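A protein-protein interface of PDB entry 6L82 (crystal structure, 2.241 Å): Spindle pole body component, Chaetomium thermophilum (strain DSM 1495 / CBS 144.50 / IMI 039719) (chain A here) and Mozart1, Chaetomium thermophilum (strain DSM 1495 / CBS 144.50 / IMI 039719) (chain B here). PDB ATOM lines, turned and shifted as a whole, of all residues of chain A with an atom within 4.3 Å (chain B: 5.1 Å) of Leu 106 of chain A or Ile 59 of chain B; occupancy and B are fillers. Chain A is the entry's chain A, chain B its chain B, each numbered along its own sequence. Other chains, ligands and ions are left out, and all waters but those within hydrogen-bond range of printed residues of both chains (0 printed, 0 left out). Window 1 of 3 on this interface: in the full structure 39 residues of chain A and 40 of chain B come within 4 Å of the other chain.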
ATOM      1  N   ILE A  23     -23.813 -15.167 -15.505  1.00  0.00           N
ATOM      2  CA  ILE A  23     -24.716 -14.940 -14.369  1.00  0.00           C
ATOM      3  C   ILE A  23     -25.348 -16.233 -13.869  1.00  0.00           C
ATOM      4  O   ILE A  23     -25.322 -16.518 -12.670  1.00  0.00           O
ATOM      5  CB  ILE A  23     -25.807 -13.902 -14.716  1.00  0.00           C
ATOM      6  CG1 ILE A  23     -25.193 -12.519 -14.838  1.00  0.00           C
ATOM      7  CG2 ILE A  23     -26.924 -13.931 -13.659  1.00  0.00           C
ATOM      8  CD1 ILE A  23     -26.142 -11.513 -15.418  1.00  0.00           C
ATOM      9  N   LEU A 102     -28.435   1.754 -14.706  1.00  0.00           N
ATOM     10  CA  LEU A 102     -28.357   0.303 -14.572  1.00  0.00           C
ATOM     11  C   LEU A 102     -27.801  -0.092 -13.212  1.00  0.00           C
ATOM     12  O   LEU A 102     -28.338  -0.994 -12.557  1.00  0.00           O
ATOM     13  CB  LEU A 102     -27.484  -0.281 -15.697  1.00  0.00           C
ATOM     14  CG  LEU A 102     -27.137  -1.765 -15.556  1.00  0.00           C
ATOM     15  CD1 LEU A 102     -28.386  -2.630 -15.735  1.00  0.00           C
ATOM     16  CD2 LEU A 102     -26.040  -2.190 -16.537  1.00  0.00           C
ATOM     17  N   LEU A 103     -26.729   0.581 -12.763  1.00  0.00           N
ATOM     18  CA  LEU A 103     -26.164   0.259 -11.450  1.00  0.00           C
ATOM     19  C   LEU A 103     -27.127   0.635 -10.329  1.00  0.00           C
ATOM     20  O   LEU A 103     -27.288  -0.126  -9.366  1.00  0.00           O
ATOM     21  CB  LEU A 103     -24.806   0.943 -11.241  1.00  0.00           C
ATOM     22  CG  LEU A 103     -23.744   0.680 -12.319  1.00  0.00           C
ATOM     23  CD1 LEU A 103     -22.436   1.386 -11.992  1.00  0.00           C
ATOM     24  CD2 LEU A 103     -23.523  -0.828 -12.536  1.00  0.00           C
ATOM     25  N   LEU A 104     -27.785   1.794 -10.438  1.00  0.00           N
ATOM     26  CA  LEU A 104     -28.814   2.144  -9.458  1.00  0.00           C
ATOM     27  C   LEU A 104     -29.887   1.061  -9.372  1.00  0.00           C
ATOM     28  O   LEU A 104     -30.347   0.723  -8.275  1.00  0.00           O
ATOM     29  CB  LEU A 104     -29.441   3.497  -9.796  1.00  0.00           C
ATOM     30  CG  LEU A 104     -28.504   4.692  -9.678  1.00  0.00           C
ATOM     31  CD1 LEU A 104     -29.109   5.940 -10.274  1.00  0.00           C
ATOM     32  CD2 LEU A 104     -28.213   4.915  -8.210  1.00  0.00           C
ATOM     33  N   GLU A 105     -30.269   0.478 -10.519  1.00  0.00           N
ATOM     34  CA  GLU A 105     -31.302  -0.555 -10.512  1.00  0.00           C
ATOM     35  C   GLU A 105     -30.811  -1.859  -9.897  1.00  0.00           C
ATOM     36  O   GLU A 105     -31.621  -2.629  -9.380  1.00  0.00           O
ATOM     37  CB  GLU A 105     -31.808  -0.814 -11.927  1.00  0.00           C
ATOM     38  CG  GLU A 105     -32.658   0.315 -12.491  1.00  0.00           C
ATOM     39  CD  GLU A 105     -33.874   0.608 -11.637  1.00  0.00           C
ATOM     40  OE1 GLU A 105     -34.049   1.776 -11.241  1.00  0.00           O
ATOM     41  OE2 GLU A 105     -34.655  -0.331 -11.366  1.00  0.00           O
ATOM     42  N   LEU A 106     -29.505  -2.136  -9.943  1.00  0.00           N
ATOM     43  CA  LEU A 106     -28.962  -3.342  -9.328  1.00  0.00           C
ATOM     44  C   LEU A 106     -28.397  -3.103  -7.931  1.00  0.00           C
ATOM     45  O   LEU A 106     -27.930  -4.054  -7.293  1.00  0.00           O
ATOM     46  CB  LEU A 106     -27.877  -3.958 -10.235  1.00  0.00           C
ATOM     47  CG  LEU A 106     -28.369  -4.432 -11.617  1.00  0.00           C
ATOM     48  CD1 LEU A 106     -27.226  -4.914 -12.529  1.00  0.00           C
ATOM     49  CD2 LEU A 106     -29.409  -5.527 -11.477  1.00  0.00           C
ATOM     50  N   ALA A 107     -28.447  -1.872  -7.425  1.00  0.00           N
ATOM     51  CA  ALA A 107     -27.794  -1.567  -6.162  1.00  0.00           C
ATOM     52  C   ALA A 107     -28.419  -2.365  -5.025  1.00  0.00           C
ATOM     53  O   ALA A 107     -29.613  -2.663  -5.040  1.00  0.00           O
ATOM     54  CB  ALA A 107     -27.890  -0.068  -5.868  1.00  0.00           C
ATOM     55  N   ASP A 108     -27.598  -2.709  -4.028  1.00  0.00           N
ATOM     56  CA  ASP A 108     -28.059  -3.523  -2.902  1.00  0.00           C
ATOM     57  C   ASP A 108     -27.293  -3.264  -1.600  1.00  0.00           C
ATOM     58  O   ASP A 108     -27.435  -2.212  -0.972  1.00  0.00           O
ATOM     59  CB  ASP A 108     -27.949  -5.001  -3.266  1.00  0.00           C
ATOM     60  CG  ASP A 108     -28.365  -5.912  -2.133  1.00  0.00           C
ATOM     61  OD1 ASP A 108     -29.208  -5.492  -1.307  1.00  0.00           O
ATOM     62  OD2 ASP A 108     -27.841  -7.048  -2.064  1.00  0.00           O
ATOM     63  N   LEU B  30     -22.031   0.526  -4.746  1.00  0.00           N
ATOM     64  CA  LEU B  30     -23.462   0.251  -4.688  1.00  0.00           C
ATOM     65  C   LEU B  30     -23.769  -1.215  -4.381  1.00  0.00           C
ATOM     66  O   LEU B  30     -24.948  -1.569  -4.271  1.00  0.00           O
ATOM     67  CB  LEU B  30     -24.120   0.675  -6.014  1.00  0.00           C
ATOM     68  CG  LEU B  30     -24.565   2.151  -6.122  1.00  0.00           C
ATOM     69  CD1 LEU B  30     -23.495   3.135  -5.679  1.00  0.00           C
ATOM     70  CD2 LEU B  30     -25.044   2.513  -7.535  1.00  0.00           C
ATOM     71  N   ASN B  31     -22.743  -2.056  -4.233  1.00  0.00           N
ATOM     72  CA  ASN B  31     -22.900  -3.493  -4.008  1.00  0.00           C
ATOM     73  C   ASN B  31     -23.792  -4.142  -5.067  1.00  0.00           C
ATOM     74  O   ASN B  31     -24.715  -4.895  -4.760  1.00  0.00           O
ATOM     75  CB  ASN B  31     -23.435  -3.775  -2.603  1.00  0.00           C
ATOM     76  CG  ASN B  31     -23.214  -5.217  -2.182  1.00  0.00           C
ATOM     77  ND2 ASN B  31     -24.056  -5.690  -1.267  1.00  0.00           N
ATOM     78  N   CYS B  32     -23.479  -3.871  -6.338  1.00  0.00           N
ATOM     79  CA  CYS B  32     -24.287  -4.368  -7.449  1.00  0.00           C
ATOM     80  C   CYS B  32     -24.098  -5.853  -7.723  1.00  0.00           C
ATOM     81  O   CYS B  32     -24.903  -6.427  -8.455  1.00  0.00           O
ATOM     82  CB  CYS B  32     -23.959  -3.591  -8.723  1.00  0.00           C
ATOM     83  SG  CYS B  32     -24.556  -1.913  -8.673  1.00  0.00           S
ATOM     84  N   LEU B  34     -21.799  -7.190  -9.620  1.00  0.00           N
ATOM     85  CA  LEU B  34     -21.290  -7.338 -10.981  1.00  0.00           C
ATOM     86  C   LEU B  34     -19.772  -7.373 -10.954  1.00  0.00           C
ATOM     87  O   LEU B  34     -19.150  -6.438 -10.453  1.00  0.00           O
ATOM     88  CB  LEU B  34     -21.714  -6.157 -11.848  1.00  0.00           C
ATOM     89  CG  LEU B  34     -23.180  -5.869 -12.056  1.00  0.00           C
ATOM     90  CD1 LEU B  34     -23.287  -4.581 -12.811  1.00  0.00           C
ATOM     91  CD2 LEU B  34     -23.794  -6.996 -12.860  1.00  0.00           C
ATOM     92  N   CYS B  42     -22.715  -5.732 -20.085  1.00  0.00           N
ATOM     93  CA  CYS B  42     -23.762  -4.726 -20.007  1.00  0.00           C
ATOM     94  C   CYS B  42     -23.414  -3.500 -20.828  1.00  0.00           C
ATOM     95  O   CYS B  42     -24.266  -2.971 -21.558  1.00  0.00           O
ATOM     96  CB  CYS B  42     -24.000  -4.337 -18.551  1.00  0.00           C
ATOM     97  SG  CYS B  42     -24.579  -5.712 -17.568  1.00  0.00           S
ATOM     98  N   ALA B  54     -34.750  -2.425 -18.675  1.00  0.00           N
ATOM     99  CA  ALA B  54     -34.976  -3.784 -19.158  1.00  0.00           C
ATOM    100  C   ALA B  54     -33.769  -4.677 -18.875  1.00  0.00           C
ATOM    101  O   ALA B  54     -33.924  -5.815 -18.411  1.00  0.00           O
ATOM    102  CB  ALA B  54     -35.312  -3.761 -20.655  1.00  0.00           C
ATOM    103  N   LEU B  55     -32.558  -4.177 -19.124  1.00  0.00           N
ATOM    104  CA  LEU B  55     -31.364  -4.971 -18.823  1.00  0.00           C
ATOM    105  C   LEU B  55     -31.316  -5.343 -17.342  1.00  0.00           C
ATOM    106  O   LEU B  55     -31.099  -6.514 -16.987  1.00  0.00           O
ATOM    107  CB  LEU B  55     -30.103  -4.202 -19.223  1.00  0.00           C
ATOM    108  CG  LEU B  55     -28.958  -4.979 -19.872  1.00  0.00           C
ATOM    109  CD1 LEU B  55     -27.622  -4.198 -19.760  1.00  0.00           C
ATOM    110  CD2 LEU B  55     -28.828  -6.389 -19.324  1.00  0.00           C
ATOM    111  N   ALA B  56     -31.499  -4.346 -16.464  1.00  0.00           N
ATOM    112  CA  ALA B  56     -31.616  -4.601 -15.031  1.00  0.00           C
ATOM    113  C   ALA B  56     -32.598  -5.730 -14.738  1.00  0.00           C
ATOM    114  O   ALA B  56     -32.296  -6.647 -13.960  1.00  0.00           O
ATOM    115  CB  ALA B  56     -32.067  -3.332 -14.303  1.00  0.00           C
ATOM    116  N   ASN B  57     -33.803  -5.656 -15.320  1.00  0.00           N
ATOM    117  CA  ASN B  57     -34.808  -6.674 -15.027  1.00  0.00           C
ATOM    118  C   ASN B  57     -34.337  -8.042 -15.510  1.00  0.00           C
ATOM    119  O   ASN B  57     -34.479  -9.047 -14.800  1.00  0.00           O
ATOM    120  CB  ASN B  57     -36.160  -6.285 -15.645  1.00  0.00           C
ATOM    121  CG  ASN B  57     -36.860  -5.158 -14.872  1.00  0.00           C
ATOM    122  OD1 ASN B  57     -36.713  -5.043 -13.659  1.00  0.00           O
ATOM    123  ND2 ASN B  57     -37.621  -4.332 -15.575  1.00  0.00           N
ATOM    124  N   VAL B  58     -33.728  -8.092 -16.699  1.00  0.00           N
ATOM    125  CA  VAL B  58     -33.200  -9.355 -17.213  1.00  0.00           C
ATOM    126  C   VAL B  58     -32.157  -9.928 -16.258  1.00  0.00           C
ATOM    127  O   VAL B  58     -32.149 -11.132 -15.969  1.00  0.00           O
ATOM    128  CB  VAL B  58     -32.626  -9.153 -18.625  1.00  0.00           C
ATOM    129  CG1 VAL B  58     -31.700 -10.319 -19.002  1.00  0.00           C
ATOM    130  CG2 VAL B  58     -33.754  -9.019 -19.624  1.00  0.00           C
ATOM    131  N   ILE B  59     -31.273  -9.075 -15.738  1.00  0.00           N
ATOM    132  CA  ILE B  59     -30.215  -9.559 -14.856  1.00  0.00           C
ATOM    133  C   ILE B  59     -30.799 -10.100 -13.554  1.00  0.00           C
ATOM    134  O   ILE B  59     -30.406 -11.182 -13.091  1.00  0.00           O
ATOM    135  CB  ILE B  59     -29.186  -8.447 -14.604  1.00  0.00           C
ATOM    136  CG1 ILE B  59     -28.386  -8.170 -15.882  1.00  0.00           C
ATOM    137  CG2 ILE B  59     -28.240  -8.858 -13.503  1.00  0.00           C
ATOM    138  CD1 ILE B  59     -27.479  -6.950 -15.748  1.00  0.00           C
ATOM    139  N   LYS B  60     -31.743  -9.360 -12.946  1.00  0.00           N
ATOM    140  CA  LYS B  60     -32.432  -9.856 -11.752  1.00  0.00           C
ATOM    141  C   LYS B  60     -33.051 -11.223 -12.014  1.00  0.00           C
ATOM    142  O   LYS B  60     -32.856 -12.167 -11.239  1.00  0.00           O
ATOM    143  CB  LYS B  60     -33.520  -8.865 -11.281  1.00  0.00           C
ATOM    144  CG  LYS B  60     -32.984  -7.551 -10.677  1.00  0.00           C
ATOM    145  CD  LYS B  60     -34.108  -6.572 -10.379  1.00  0.00           C
ATOM    146  CE  LYS B  60     -33.582  -5.161 -10.170  1.00  0.00           C
ATOM    147  NZ  LYS B  60     -34.592  -4.244  -9.542  1.00  0.00           N
ATOM    148  N   GLU B  61     -33.779 -11.356 -13.125  1.00  0.00           N
ATOM    149  CA  GLU B  61     -34.421 -12.630 -13.427  1.00  0.00           C
ATOM    150  C   GLU B  61     -33.387 -13.732 -13.633  1.00  0.00           C
ATOM    151  O   GLU B  61     -33.576 -14.865 -13.170  1.00  0.00           O
ATOM    152  CB  GLU B  61     -35.312 -12.482 -14.652  1.00  0.00           C
ATOM    153  CG  GLU B  61     -36.061 -13.743 -15.021  1.00  0.00           C
ATOM    154  CD  GLU B  61     -37.075 -14.174 -13.967  1.00  0.00           C
ATOM    155  OE1 GLU B  61     -37.256 -15.393 -13.812  1.00  0.00           O
ATOM    156  OE2 GLU B  61     -37.697 -13.314 -13.312  1.00  0.00           O
ATOM    157  N   LEU B  62     -32.269 -13.413 -14.299  1.00  0.00           N
ATOM    158  CA  LEU B  62     -31.227 -14.418 -14.498  1.00  0.00           C
ATOM    159  C   LEU B  62     -30.668 -14.888 -13.166  1.00  0.00           C
ATOM    160  O   LEU B  62     -30.385 -16.079 -12.985  1.00  0.00           O
ATOM    161  CB  LEU B  62     -30.114 -13.856 -15.374  1.00  0.00           C
ATOM    162  CG  LEU B  62     -30.517 -13.718 -16.838  1.00  0.00           C
ATOM    163  CD1 LEU B  62     -29.315 -13.284 -17.642  1.00  0.00           C
ATOM    164  CD2 LEU B  62     -31.042 -15.049 -17.335  1.00  0.00           C
ATOM    165  N   ARG B  63     -30.548 -13.967 -12.206  1.00  0.00           N
ATOM    166  CA  ARG B  63     -30.070 -14.321 -10.873  1.00  0.00           C
ATOM    167  C   ARG B  63     -31.033 -15.261 -10.158  1.00  0.00           C
ATOM    168  O   ARG B  63     -30.596 -16.219  -9.516  1.00  0.00           O
ATOM    169  CB  ARG B  63     -29.829 -13.049 -10.055  1.00  0.00           C
ATOM    170  CG  ARG B  63     -28.524 -12.346 -10.481  1.00  0.00           C
ATOM    171  CD  ARG B  63     -28.373 -10.965  -9.888  1.00  0.00           C
ATOM    172  NE  ARG B  63     -27.076 -10.380 -10.229  1.00  0.00           N
ATOM    173  CZ  ARG B  63     -26.682  -9.176  -9.830  1.00  0.00           C
ATOM    174  NH1 ARG B  63     -27.490  -8.439  -9.070  1.00  0.00           N
ATOM    175  NH2 ARG B  63     -25.480  -8.713 -10.168  1.00  0.00           N
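O of Leu 103 of chain A lies within hydrogen-bond range of SG of Cys 32 of chain B (3.3 Å). The side-chain amino group of Lys 60 of chain B lies close to the backbone carbonyl oxygen of Glu 105 of chain A (3.4 Å). N of Asp 108 of chain A sits at hydrogen-bond distance from O of Leu 30 of chain B (2.9 Å).
The backbone carbonyl oxygen (O) of Cys 32 of chain B lies within hydrogen-bond range of the guanidinium group (NH2) of Arg 63 of chain B, at 2.9 Å.
Leu 106 of chain A touches just these residues of chain B: Cys 32 (3.7 Å), Leu 34 (3.96 Å), Ala 56 (3.97 Å) and Ile 59 (3.8 Å). Printed residues of chain A within 4 Å of Asn 31 of chain B: Asp 108. Ala 54 of chain B touches none of the printed residues of chain A. Leu 55 of chain B touches none of the printed residues of chain A. Printed residues of chain A within 4 Å of Ala 56 of chain B: Leu 102, Glu 105 and Leu 106. Ile 59 of chain B touches just these residues of chain A: Ile 23 and Leu 106. The nearest printed residue of chain B that does not touch Leu 106 of chain A is Asn 31 of chain B (4.2 Å). The nearest printed residue of chain A that does not touch Ile 59 of chain B is Leu 102 of chain A (4.4 Å).
Ile 23 of chain A touches Ile 59 of chain B (CD1 to CG2, 3.9 Å). Leu 62 of chain B touches Ile 23 of chain A (CB to CG2, 3.6 Å). Arg 63 of chain B touches Ile 23 of chain A (CG to CG2, 3.9 Å). CB of Cys 42 of chain B touches CD2 of Leu 102 of chain A (3.6 Å). Leu 30 of chain B touches Leu 103 of chain A (CD2 to O, 3.9 Å). Ala 56 of chain B touches Glu 105 of chain A (CB to CB, 3.5 Å). Leu 34 of chain B touches Leu 106 of chain A (CD1 to CD1, 3.96 Å). CD1 of Leu 106 of chain A touches CD1 of Ile 59 of chain B (3.8 Å). O of Leu 30 of chain B touches CA of Ala 107 of chain A, at 3.4 Å. Asn 31 of chain B touches Asp 108 of chain A.
Hydrophobic or aromatic side chains of chain B that line the printed part of chain A: Leu 30, Leu 34, Ala 56, Ile 59 and Leu 62. Of the 8 printed residues of chain A, 7 touch a printed residue of chain B. Among the printed residues, no Asp or Glu carboxylate lies within 4 Å of a Lys or Arg side-chain nitrogen of the other chain.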
